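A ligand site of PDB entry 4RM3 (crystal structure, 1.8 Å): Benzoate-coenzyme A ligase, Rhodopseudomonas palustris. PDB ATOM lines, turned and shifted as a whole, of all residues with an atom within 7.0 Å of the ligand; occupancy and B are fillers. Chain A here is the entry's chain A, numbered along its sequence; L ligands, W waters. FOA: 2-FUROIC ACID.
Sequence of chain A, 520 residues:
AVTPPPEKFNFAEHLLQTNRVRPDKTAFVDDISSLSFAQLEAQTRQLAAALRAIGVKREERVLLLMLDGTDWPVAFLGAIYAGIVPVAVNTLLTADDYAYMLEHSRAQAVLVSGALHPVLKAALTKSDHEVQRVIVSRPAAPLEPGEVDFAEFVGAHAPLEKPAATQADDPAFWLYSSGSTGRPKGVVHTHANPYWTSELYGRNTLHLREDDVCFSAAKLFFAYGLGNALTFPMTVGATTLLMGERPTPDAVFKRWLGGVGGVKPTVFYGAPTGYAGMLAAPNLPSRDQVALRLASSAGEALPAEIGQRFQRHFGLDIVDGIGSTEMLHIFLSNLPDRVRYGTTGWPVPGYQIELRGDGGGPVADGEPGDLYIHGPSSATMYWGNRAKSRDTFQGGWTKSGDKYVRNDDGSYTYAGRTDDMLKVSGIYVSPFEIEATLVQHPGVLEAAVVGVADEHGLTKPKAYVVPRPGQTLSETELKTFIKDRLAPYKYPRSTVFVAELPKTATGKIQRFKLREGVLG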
ATOM      1  N   PHE A 222     -25.798  -8.315  15.288  1.00  0.00           N
ATOM      2  CA  PHE A 222     -26.289  -9.079  14.105  1.00  0.00           C
ATOM      3  C   PHE A 222     -25.601  -8.575  12.861  1.00  0.00           C
ATOM      4  O   PHE A 222     -25.519  -7.423  12.684  1.00  0.00           O
ATOM      5  CB  PHE A 222     -27.752  -8.946  13.914  1.00  0.00           C
ATOM      6  CG  PHE A 222     -28.614  -9.667  14.999  1.00  0.00           C
ATOM      7  CD1 PHE A 222     -28.796 -11.065  14.982  1.00  0.00           C
ATOM      8  CD2 PHE A 222     -29.227  -8.929  16.012  1.00  0.00           C
ATOM      9  CE1 PHE A 222     -29.605 -11.721  15.976  1.00  0.00           C
ATOM     10  CE2 PHE A 222     -30.093  -9.542  16.992  1.00  0.00           C
ATOM     11  CZ  PHE A 222     -30.264 -10.920  16.997  1.00  0.00           C
ATOM     12  N   ALA A 223     -25.234  -9.473  11.929  1.00  0.00           N
ATOM     13  CA  ALA A 223     -24.750  -8.954  10.657  1.00  0.00           C
ATOM     14  C   ALA A 223     -25.790  -7.922  10.094  1.00  0.00           C
ATOM     15  O   ALA A 223     -25.402  -6.872   9.512  1.00  0.00           O
ATOM     16  CB  ALA A 223     -24.640 -10.127   9.743  1.00  0.00           C
ATOM     17  N   TYR A 224     -27.067  -8.276  10.147  1.00  0.00           N
ATOM     18  CA  TYR A 224     -28.099  -7.422   9.528  1.00  0.00           C
ATOM     19  C   TYR A 224     -28.028  -6.063  10.198  1.00  0.00           C
ATOM     20  O   TYR A 224     -27.927  -5.001   9.561  1.00  0.00           O
ATOM     21  CB  TYR A 224     -29.445  -8.071   9.858  1.00  0.00           C
ATOM     22  CG  TYR A 224     -30.691  -7.336   9.323  1.00  0.00           C
ATOM     23  CD1 TYR A 224     -30.700  -6.825   8.007  1.00  0.00           C
ATOM     24  CD2 TYR A 224     -31.873  -7.257  10.121  1.00  0.00           C
ATOM     25  CE1 TYR A 224     -31.879  -6.173   7.515  1.00  0.00           C
ATOM     26  CE2 TYR A 224     -33.023  -6.592   9.666  1.00  0.00           C
ATOM     27  CZ  TYR A 224     -33.009  -6.035   8.400  1.00  0.00           C
ATOM     28  OH  TYR A 224     -34.140  -5.396   7.913  1.00  0.00           O
ATOM     29  N   GLY A 225     -28.016  -6.106  11.529  1.00  0.00           N
ATOM     30  CA  GLY A 225     -27.952  -4.836  12.279  1.00  0.00           C
ATOM     31  C   GLY A 225     -26.699  -3.973  12.112  1.00  0.00           C
ATOM     32  O   GLY A 225     -26.767  -2.702  12.111  1.00  0.00           O
ATOM     33  N   ASN A 228     -27.271  -2.102   9.064  1.00  0.00           N
ATOM     34  CA  ASN A 228     -28.376  -1.203   9.082  1.00  0.00           C
ATOM     35  C   ASN A 228     -28.052   0.016   9.906  1.00  0.00           C
ATOM     36  O   ASN A 228     -28.447   1.114   9.592  1.00  0.00           O
ATOM     37  CB  ASN A 228     -29.523  -1.958   9.820  1.00  0.00           C
ATOM     38  CG  ASN A 228     -30.064  -3.149   9.122  1.00  0.00           C
ATOM     39  OD1 ASN A 228     -29.805  -3.417   7.933  1.00  0.00           O
ATOM     40  ND2 ASN A 228     -30.897  -3.951   9.903  1.00  0.00           N
ATOM     41  N   SER A 297     -36.845  -5.519   6.100  1.00  0.00           N
ATOM     42  CA  SER A 297     -37.066  -6.749   6.836  1.00  0.00           C
ATOM     43  C   SER A 297     -36.050  -7.837   6.456  1.00  0.00           C
ATOM     44  O   SER A 297     -35.793  -8.085   5.278  1.00  0.00           O
ATOM     45  CB  SER A 297     -38.467  -7.316   6.498  1.00  0.00           C
ATOM     46  OG  SER A 297     -38.645  -8.419   7.311  1.00  0.00           O
ATOM     47  N   ALA A 298     -35.544  -8.541   7.467  1.00  0.00           N
ATOM     48  CA  ALA A 298     -34.749  -9.700   7.224  1.00  0.00           C
ATOM     49  C   ALA A 298     -34.690 -10.493   8.496  1.00  0.00           C
ATOM     50  O   ALA A 298     -35.033  -9.967   9.551  1.00  0.00           O
ATOM     51  CB  ALA A 298     -33.346  -9.375   6.767  1.00  0.00           C
ATOM     52  N   GLY A 299     -34.192 -11.723   8.422  1.00  0.00           N
ATOM     53  CA  GLY A 299     -34.022 -12.556   9.675  1.00  0.00           C
ATOM     54  C   GLY A 299     -35.002 -13.744   9.681  1.00  0.00           C
ATOM     55  O   GLY A 299     -34.819 -14.709  10.456  1.00  0.00           O
ATOM     56  N   GLU A 300     -36.014 -13.699   8.824  1.00  0.00           N
ATOM     57  CA  GLU A 300     -36.758 -14.937   8.419  1.00  0.00           C
ATOM     58  C   GLU A 300     -37.556 -14.526   7.180  1.00  0.00           C
ATOM     59  O   GLU A 300     -37.591 -13.332   6.896  1.00  0.00           O
ATOM     60  CB  GLU A 300     -37.741 -15.371   9.490  1.00  0.00           C
ATOM     61  CG  GLU A 300     -38.550 -14.217   9.938  1.00  0.00           C
ATOM     62  CD  GLU A 300     -39.190 -14.385  11.315  1.00  0.00           C
ATOM     63  OE1 GLU A 300     -39.575 -15.555  11.685  1.00  0.00           O
ATOM     64  OE2 GLU A 300     -39.357 -13.333  11.962  1.00  0.00           O
ATOM     65  N   ASP A 320     -38.314  -6.898   2.009  1.00  0.00           N
ATOM     66  CA  ASP A 320     -37.750  -8.089   2.638  1.00  0.00           C
ATOM     67  C   ASP A 320     -36.651  -8.702   1.784  1.00  0.00           C
ATOM     68  O   ASP A 320     -36.867  -9.048   0.625  1.00  0.00           O
ATOM     69  CB  ASP A 320     -38.844  -9.117   2.912  1.00  0.00           C
ATOM     70  CG  ASP A 320     -38.340 -10.543   2.797  1.00  0.00           C
ATOM     71  OD1 ASP A 320     -37.216 -10.817   3.251  1.00  0.00           O
ATOM     72  OD2 ASP A 320     -39.079 -11.390   2.238  1.00  0.00           O
ATOM     73  N   GLY A 321     -35.467  -8.837   2.379  1.00  0.00           N
ATOM     74  CA  GLY A 321     -34.309  -9.480   1.666  1.00  0.00           C
ATOM     75  C   GLY A 321     -33.653 -10.527   2.628  1.00  0.00           C
ATOM     76  O   GLY A 321     -33.998 -10.642   3.811  1.00  0.00           O
ATOM     77  N   ILE A 322     -32.729 -11.315   2.085  1.00  0.00           N
ATOM     78  CA  ILE A 322     -32.094 -12.373   2.858  1.00  0.00           C
ATOM     79  C   ILE A 322     -30.564 -12.092   2.758  1.00  0.00           C
ATOM     80  O   ILE A 322     -30.066 -11.877   1.674  1.00  0.00           O
ATOM     81  CB  ILE A 322     -32.428 -13.818   2.352  1.00  0.00           C
ATOM     82  CG1 ILE A 322     -31.680 -14.815   3.307  1.00  0.00           C
ATOM     83  CG2 ILE A 322     -32.056 -14.008   0.844  1.00  0.00           C
ATOM     84  CD1 ILE A 322     -32.323 -16.292   3.369  1.00  0.00           C
ATOM     85  N   GLY A 323     -29.871 -12.092   3.889  1.00  0.00           N
ATOM     86  CA  GLY A 323     -28.412 -12.181   3.847  1.00  0.00           C
ATOM     87  C   GLY A 323     -27.934 -13.274   4.786  1.00  0.00           C
ATOM     88  O   GLY A 323     -28.715 -14.155   5.232  1.00  0.00           O
ATOM     89  N   SER A 324     -26.639 -13.307   5.044  1.00  0.00           N
ATOM     90  CA  SER A 324     -26.224 -14.235   6.130  1.00  0.00           C
ATOM     91  C   SER A 324     -25.066 -13.672   6.884  1.00  0.00           C
ATOM     92  O   SER A 324     -24.492 -12.681   6.451  1.00  0.00           O
ATOM     93  CB  SER A 324     -25.837 -15.608   5.513  1.00  0.00           C
ATOM     94  OG  SER A 324     -24.701 -15.455   4.648  1.00  0.00           O
ATOM     95  N   THR A 325     -24.680 -14.339   7.991  1.00  0.00           N
ATOM     96  CA  THR A 325     -23.465 -13.925   8.699  1.00  0.00           C
ATOM     97  C   THR A 325     -22.229 -14.038   7.797  1.00  0.00           C
ATOM     98  O   THR A 325     -21.411 -13.126   7.725  1.00  0.00           O
ATOM     99  CB  THR A 325     -23.288 -14.810   9.965  1.00  0.00           C
ATOM    100  OG1 THR A 325     -24.515 -14.726  10.725  1.00  0.00           O
ATOM    101  CG2 THR A 325     -22.118 -14.296  10.791  1.00  0.00           C
ATOM    102  N   MET A 327     -22.175 -14.031   4.411  1.00  0.00           N
ATOM    103  CA  MET A 327     -22.149 -13.009   3.336  1.00  0.00           C
ATOM    104  C   MET A 327     -22.193 -11.590   3.848  1.00  0.00           C
ATOM    105  O   MET A 327     -22.093 -10.704   3.054  1.00  0.00           O
ATOM    106  CB  MET A 327     -23.303 -13.219   2.320  1.00  0.00           C
ATOM    107  CG  MET A 327     -23.260 -14.532   1.529  1.00  0.00           C
ATOM    108  SD  MET A 327     -21.622 -14.717   0.690  1.00  0.00           S
ATOM    109  CE  MET A 327     -21.618 -13.275  -0.383  1.00  0.00           C
ATOM    110  N   LEU A 328     -22.307 -11.394   5.176  1.00  0.00           N
ATOM    111  CA  LEU A 328     -22.242 -10.082   5.819  1.00  0.00           C
ATOM    112  C   LEU A 328     -23.542  -9.291   5.736  1.00  0.00           C
ATOM    113  O   LEU A 328     -23.976  -8.702   6.754  1.00  0.00           O
ATOM    114  CB  LEU A 328     -21.020  -9.176   5.436  1.00  0.00           C
ATOM    115  CG  LEU A 328     -20.791  -7.955   6.380  1.00  0.00           C
ATOM    116  CD1 LEU A 328     -20.673  -8.435   7.875  1.00  0.00           C
ATOM    117  CD2 LEU A 328     -19.643  -7.100   5.954  1.00  0.00           C
ATOM    118  N   HIS A 329     -24.177  -9.221   4.573  1.00  0.00           N
ATOM    119  CA  HIS A 329     -25.526  -8.603   4.535  1.00  0.00           C
ATOM    120  C   HIS A 329     -26.309  -9.185   3.358  1.00  0.00           C
ATOM    121  O   HIS A 329     -26.002 -10.243   2.852  1.00  0.00           O
ATOM    122  CB  HIS A 329     -25.406  -7.060   4.464  1.00  0.00           C
ATOM    123  CG  HIS A 329     -26.547  -6.344   5.158  1.00  0.00           C
ATOM    124  ND1 HIS A 329     -27.740  -6.036   4.536  1.00  0.00           N
ATOM    125  CD2 HIS A 329     -26.628  -5.787   6.402  1.00  0.00           C
ATOM    126  CE1 HIS A 329     -28.561  -5.401   5.371  1.00  0.00           C
ATOM    127  NE2 HIS A 329     -27.903  -5.224   6.536  1.00  0.00           N
ATOM    128  N   ILE A 330     -27.283  -8.442   2.879  1.00  0.00           N
ATOM    129  CA  ILE A 330     -28.295  -8.990   2.012  1.00  0.00           C
ATOM    130  C   ILE A 330     -27.777  -9.135   0.568  1.00  0.00           C
ATOM    131  O   ILE A 330     -27.221  -8.248  -0.022  1.00  0.00           O
ATOM    132  CB  ILE A 330     -29.581  -8.060   2.100  1.00  0.00           C
ATOM    133  CG1 ILE A 330     -30.287  -8.288   3.415  1.00  0.00           C
ATOM    134  CG2 ILE A 330     -30.548  -8.360   0.981  1.00  0.00           C
ATOM    135  CD1 ILE A 330     -31.396  -7.287   3.844  1.00  0.00           C
ATOM    136  N   PHE A 331     -28.082 -10.285  -0.021  1.00  0.00           N
ATOM    137  CA  PHE A 331     -27.675 -10.552  -1.401  1.00  0.00           C
ATOM    138  C   PHE A 331     -28.819 -10.865  -2.329  1.00  0.00           C
ATOM    139  O   PHE A 331     -28.595 -11.019  -3.537  1.00  0.00           O
ATOM    140  CB  PHE A 331     -26.620 -11.699  -1.367  1.00  0.00           C
ATOM    141  CG  PHE A 331     -27.042 -12.883  -0.544  1.00  0.00           C
ATOM    142  CD1 PHE A 331     -28.104 -13.715  -1.019  1.00  0.00           C
ATOM    143  CD2 PHE A 331     -26.464 -13.147   0.695  1.00  0.00           C
ATOM    144  CE1 PHE A 331     -28.511 -14.849  -0.285  1.00  0.00           C
ATOM    145  CE2 PHE A 331     -26.959 -14.226   1.509  1.00  0.00           C
ATOM    146  CZ  PHE A 331     -27.971 -15.097   1.020  1.00  0.00           C
ATOM    147  N   LYS A 423     -35.010 -20.669  11.881  1.00  0.00           N
ATOM    148  CA  LYS A 423     -34.665 -19.269  11.943  1.00  0.00           C
ATOM    149  C   LYS A 423     -35.781 -18.507  12.613  1.00  0.00           C
ATOM    150  O   LYS A 423     -36.797 -18.222  11.990  1.00  0.00           O
ATOM    151  CB  LYS A 423     -34.350 -18.724  10.556  1.00  0.00           C
ATOM    152  CG  LYS A 423     -33.174 -17.797  10.587  1.00  0.00           C
ATOM    153  CD  LYS A 423     -32.882 -17.218   9.189  1.00  0.00           C
ATOM    154  CE  LYS A 423     -32.027 -15.921   9.327  1.00  0.00           C
ATOM    155  NZ  LYS A 423     -31.793 -15.411   7.887  1.00  0.00           N
ATOM    156  N   GLY A 426     -34.829 -13.813  13.316  1.00  0.00           N
ATOM    157  CA  GLY A 426     -33.449 -13.364  13.144  1.00  0.00           C
ATOM    158  C   GLY A 426     -32.332 -14.184  13.755  1.00  0.00           C
ATOM    159  O   GLY A 426     -31.169 -13.972  13.443  1.00  0.00           O
ATOM    160  N   ILE A 427     -32.672 -15.083  14.670  1.00  0.00           N
ATOM    161  CA  ILE A 427     -31.638 -15.881  15.347  1.00  0.00           C
ATOM    162  C   ILE A 427     -31.883 -17.343  15.021  1.00  0.00           C
ATOM    163  O   ILE A 427     -33.013 -17.850  15.149  1.00  0.00           O
ATOM    164  CB  ILE A 427     -31.589 -15.683  16.907  1.00  0.00           C
ATOM    165  CG1 ILE A 427     -31.423 -14.213  17.298  1.00  0.00           C
ATOM    166  CG2 ILE A 427     -30.432 -16.406  17.555  1.00  0.00           C
ATOM    167  CD1 ILE A 427     -32.233 -13.780  18.583  1.00  0.00           C
ATOM    168  N   TYR A 428     -30.807 -18.000  14.602  1.00  0.00           N
ATOM    169  CA  TYR A 428     -30.771 -19.377  14.360  1.00  0.00           C
ATOM    170  C   TYR A 428     -30.911 -20.107  15.704  1.00  0.00           C
ATOM    171  O   TYR A 428     -30.200 -19.790  16.660  1.00  0.00           O
ATOM    172  CB  TYR A 428     -29.484 -19.698  13.632  1.00  0.00           C
ATOM    173  CG  TYR A 428     -29.600 -19.444  12.167  1.00  0.00           C
ATOM    174  CD1 TYR A 428     -30.384 -20.286  11.383  1.00  0.00           C
ATOM    175  CD2 TYR A 428     -28.972 -18.350  11.528  1.00  0.00           C
ATOM    176  CE1 TYR A 428     -30.541 -20.108  10.004  1.00  0.00           C
ATOM    177  CE2 TYR A 428     -29.136 -18.158  10.101  1.00  0.00           C
ATOM    178  CZ  TYR A 428     -29.916 -19.069   9.382  1.00  0.00           C
ATOM    179  OH  TYR A 428     -30.164 -18.967   8.030  1.00  0.00           O
HETATM  180  C1  FOA L   1     -30.428 -12.229   7.422  1.00  0.00           C
HETATM  181  C2  FOA L   1     -29.374 -11.165   7.226  1.00  0.00           C
HETATM  182  C3  FOA L   1     -29.551  -9.977   6.598  1.00  0.00           C
HETATM  183  C4  FOA L   1     -28.380  -9.304   6.605  1.00  0.00           C
HETATM  184  C5  FOA L   1     -27.503 -10.062   7.331  1.00  0.00           C
HETATM  185  O6  FOA L   1     -30.507 -12.998   8.427  1.00  0.00           O
HETATM  186  O7  FOA L   1     -31.307 -12.308   6.506  1.00  0.00           O
HETATM  187  O8  FOA L   1     -28.082 -11.264   7.745  1.00  0.00           O
HETATM  188  O   HOH W   1     -28.026 -10.911  11.165  1.00  0.00           O
HETATM  189  O   HOH W   2     -33.819 -12.806   5.653  1.00  0.00           O
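An oxygen (O7) of the ligand is in hydrogen-bond range of the backbone NH of Gly 323.
The side-chain amino group (NZ) of Lys 423 lies within salt-bridge range of an oxygen (O6) of the ligand.
Ala 223 touches the ligand (CB to C5, 3.7 Å).
Tyr 224 touches the ligand (N to C5, 3.4 Å).
Ala 298 touches the ligand (CB to O7, 3.6 Å).
Gly 299 touches the ligand (N to O7, 3.5 Å).
Ile 322 touches the ligand (CA to O7, 3.7 Å).
Ser 324 touches the ligand.
Leu 328 touches the ligand (O to C5, 3.8 Å).
His 329 touches the ligand (CA to C4, 3.6 Å).
CG1 of Ile 330 touches C3 of the ligand, at 3.7 Å.
Within 4 Å of the ligand: Ala 223, Tyr 224, Ala 298, Gly 299, Ile 322, Gly 323, Ser 324, Leu 328, His 329, Ile 330 and Lys 423.
Water W2 lies within hydrogen-bond range of an oxygen (O7) of the ligand (2.7 Å), the backbone carbonyl oxygen (O) of Gly 321 (2.8 Å) and the backbone NH (N) of Gly 299 (3.0 Å).
Water W1 lies within hydrogen-bond range of N of Tyr 224, N of Ala 223 and O8 of the ligand.
The backbone carbonyl oxygen (O) of Tyr 224 sits close to the side-chain amide oxygen (OD1) of Asn 228, at 2.9 Å.
OH of Tyr 224 sits at hydrogen-bond distance from N of Ala 298 (3.5 Å).
The backbone NH (N) of Ser 297 sits at hydrogen-bond distance from the side-chain hydroxyl (OH) of Tyr 224 (3.3 Å).
The backbone NH of Met 327 sits at hydrogen-bond distance from the side-chain hydroxyl of Ser 324 (2.9 Å).
N of Phe 331 sits at hydrogen-bond distance from O of Ile 322, at 3.1 Å.
The backbone NH of Gly 426 is in hydrogen-bond range of the backbone carbonyl oxygen of Gly 299, at 3.0 Å.
The backbone carbonyl oxygen (O) of Tyr 224 lies within hydrogen-bond range of a ring nitrogen (NE2) of His 329 (3.0 Å).
The side-chain amide oxygen (OD1) of Asn 228 is in hydrogen-bond range of a ring nitrogen (NE2) of His 329.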
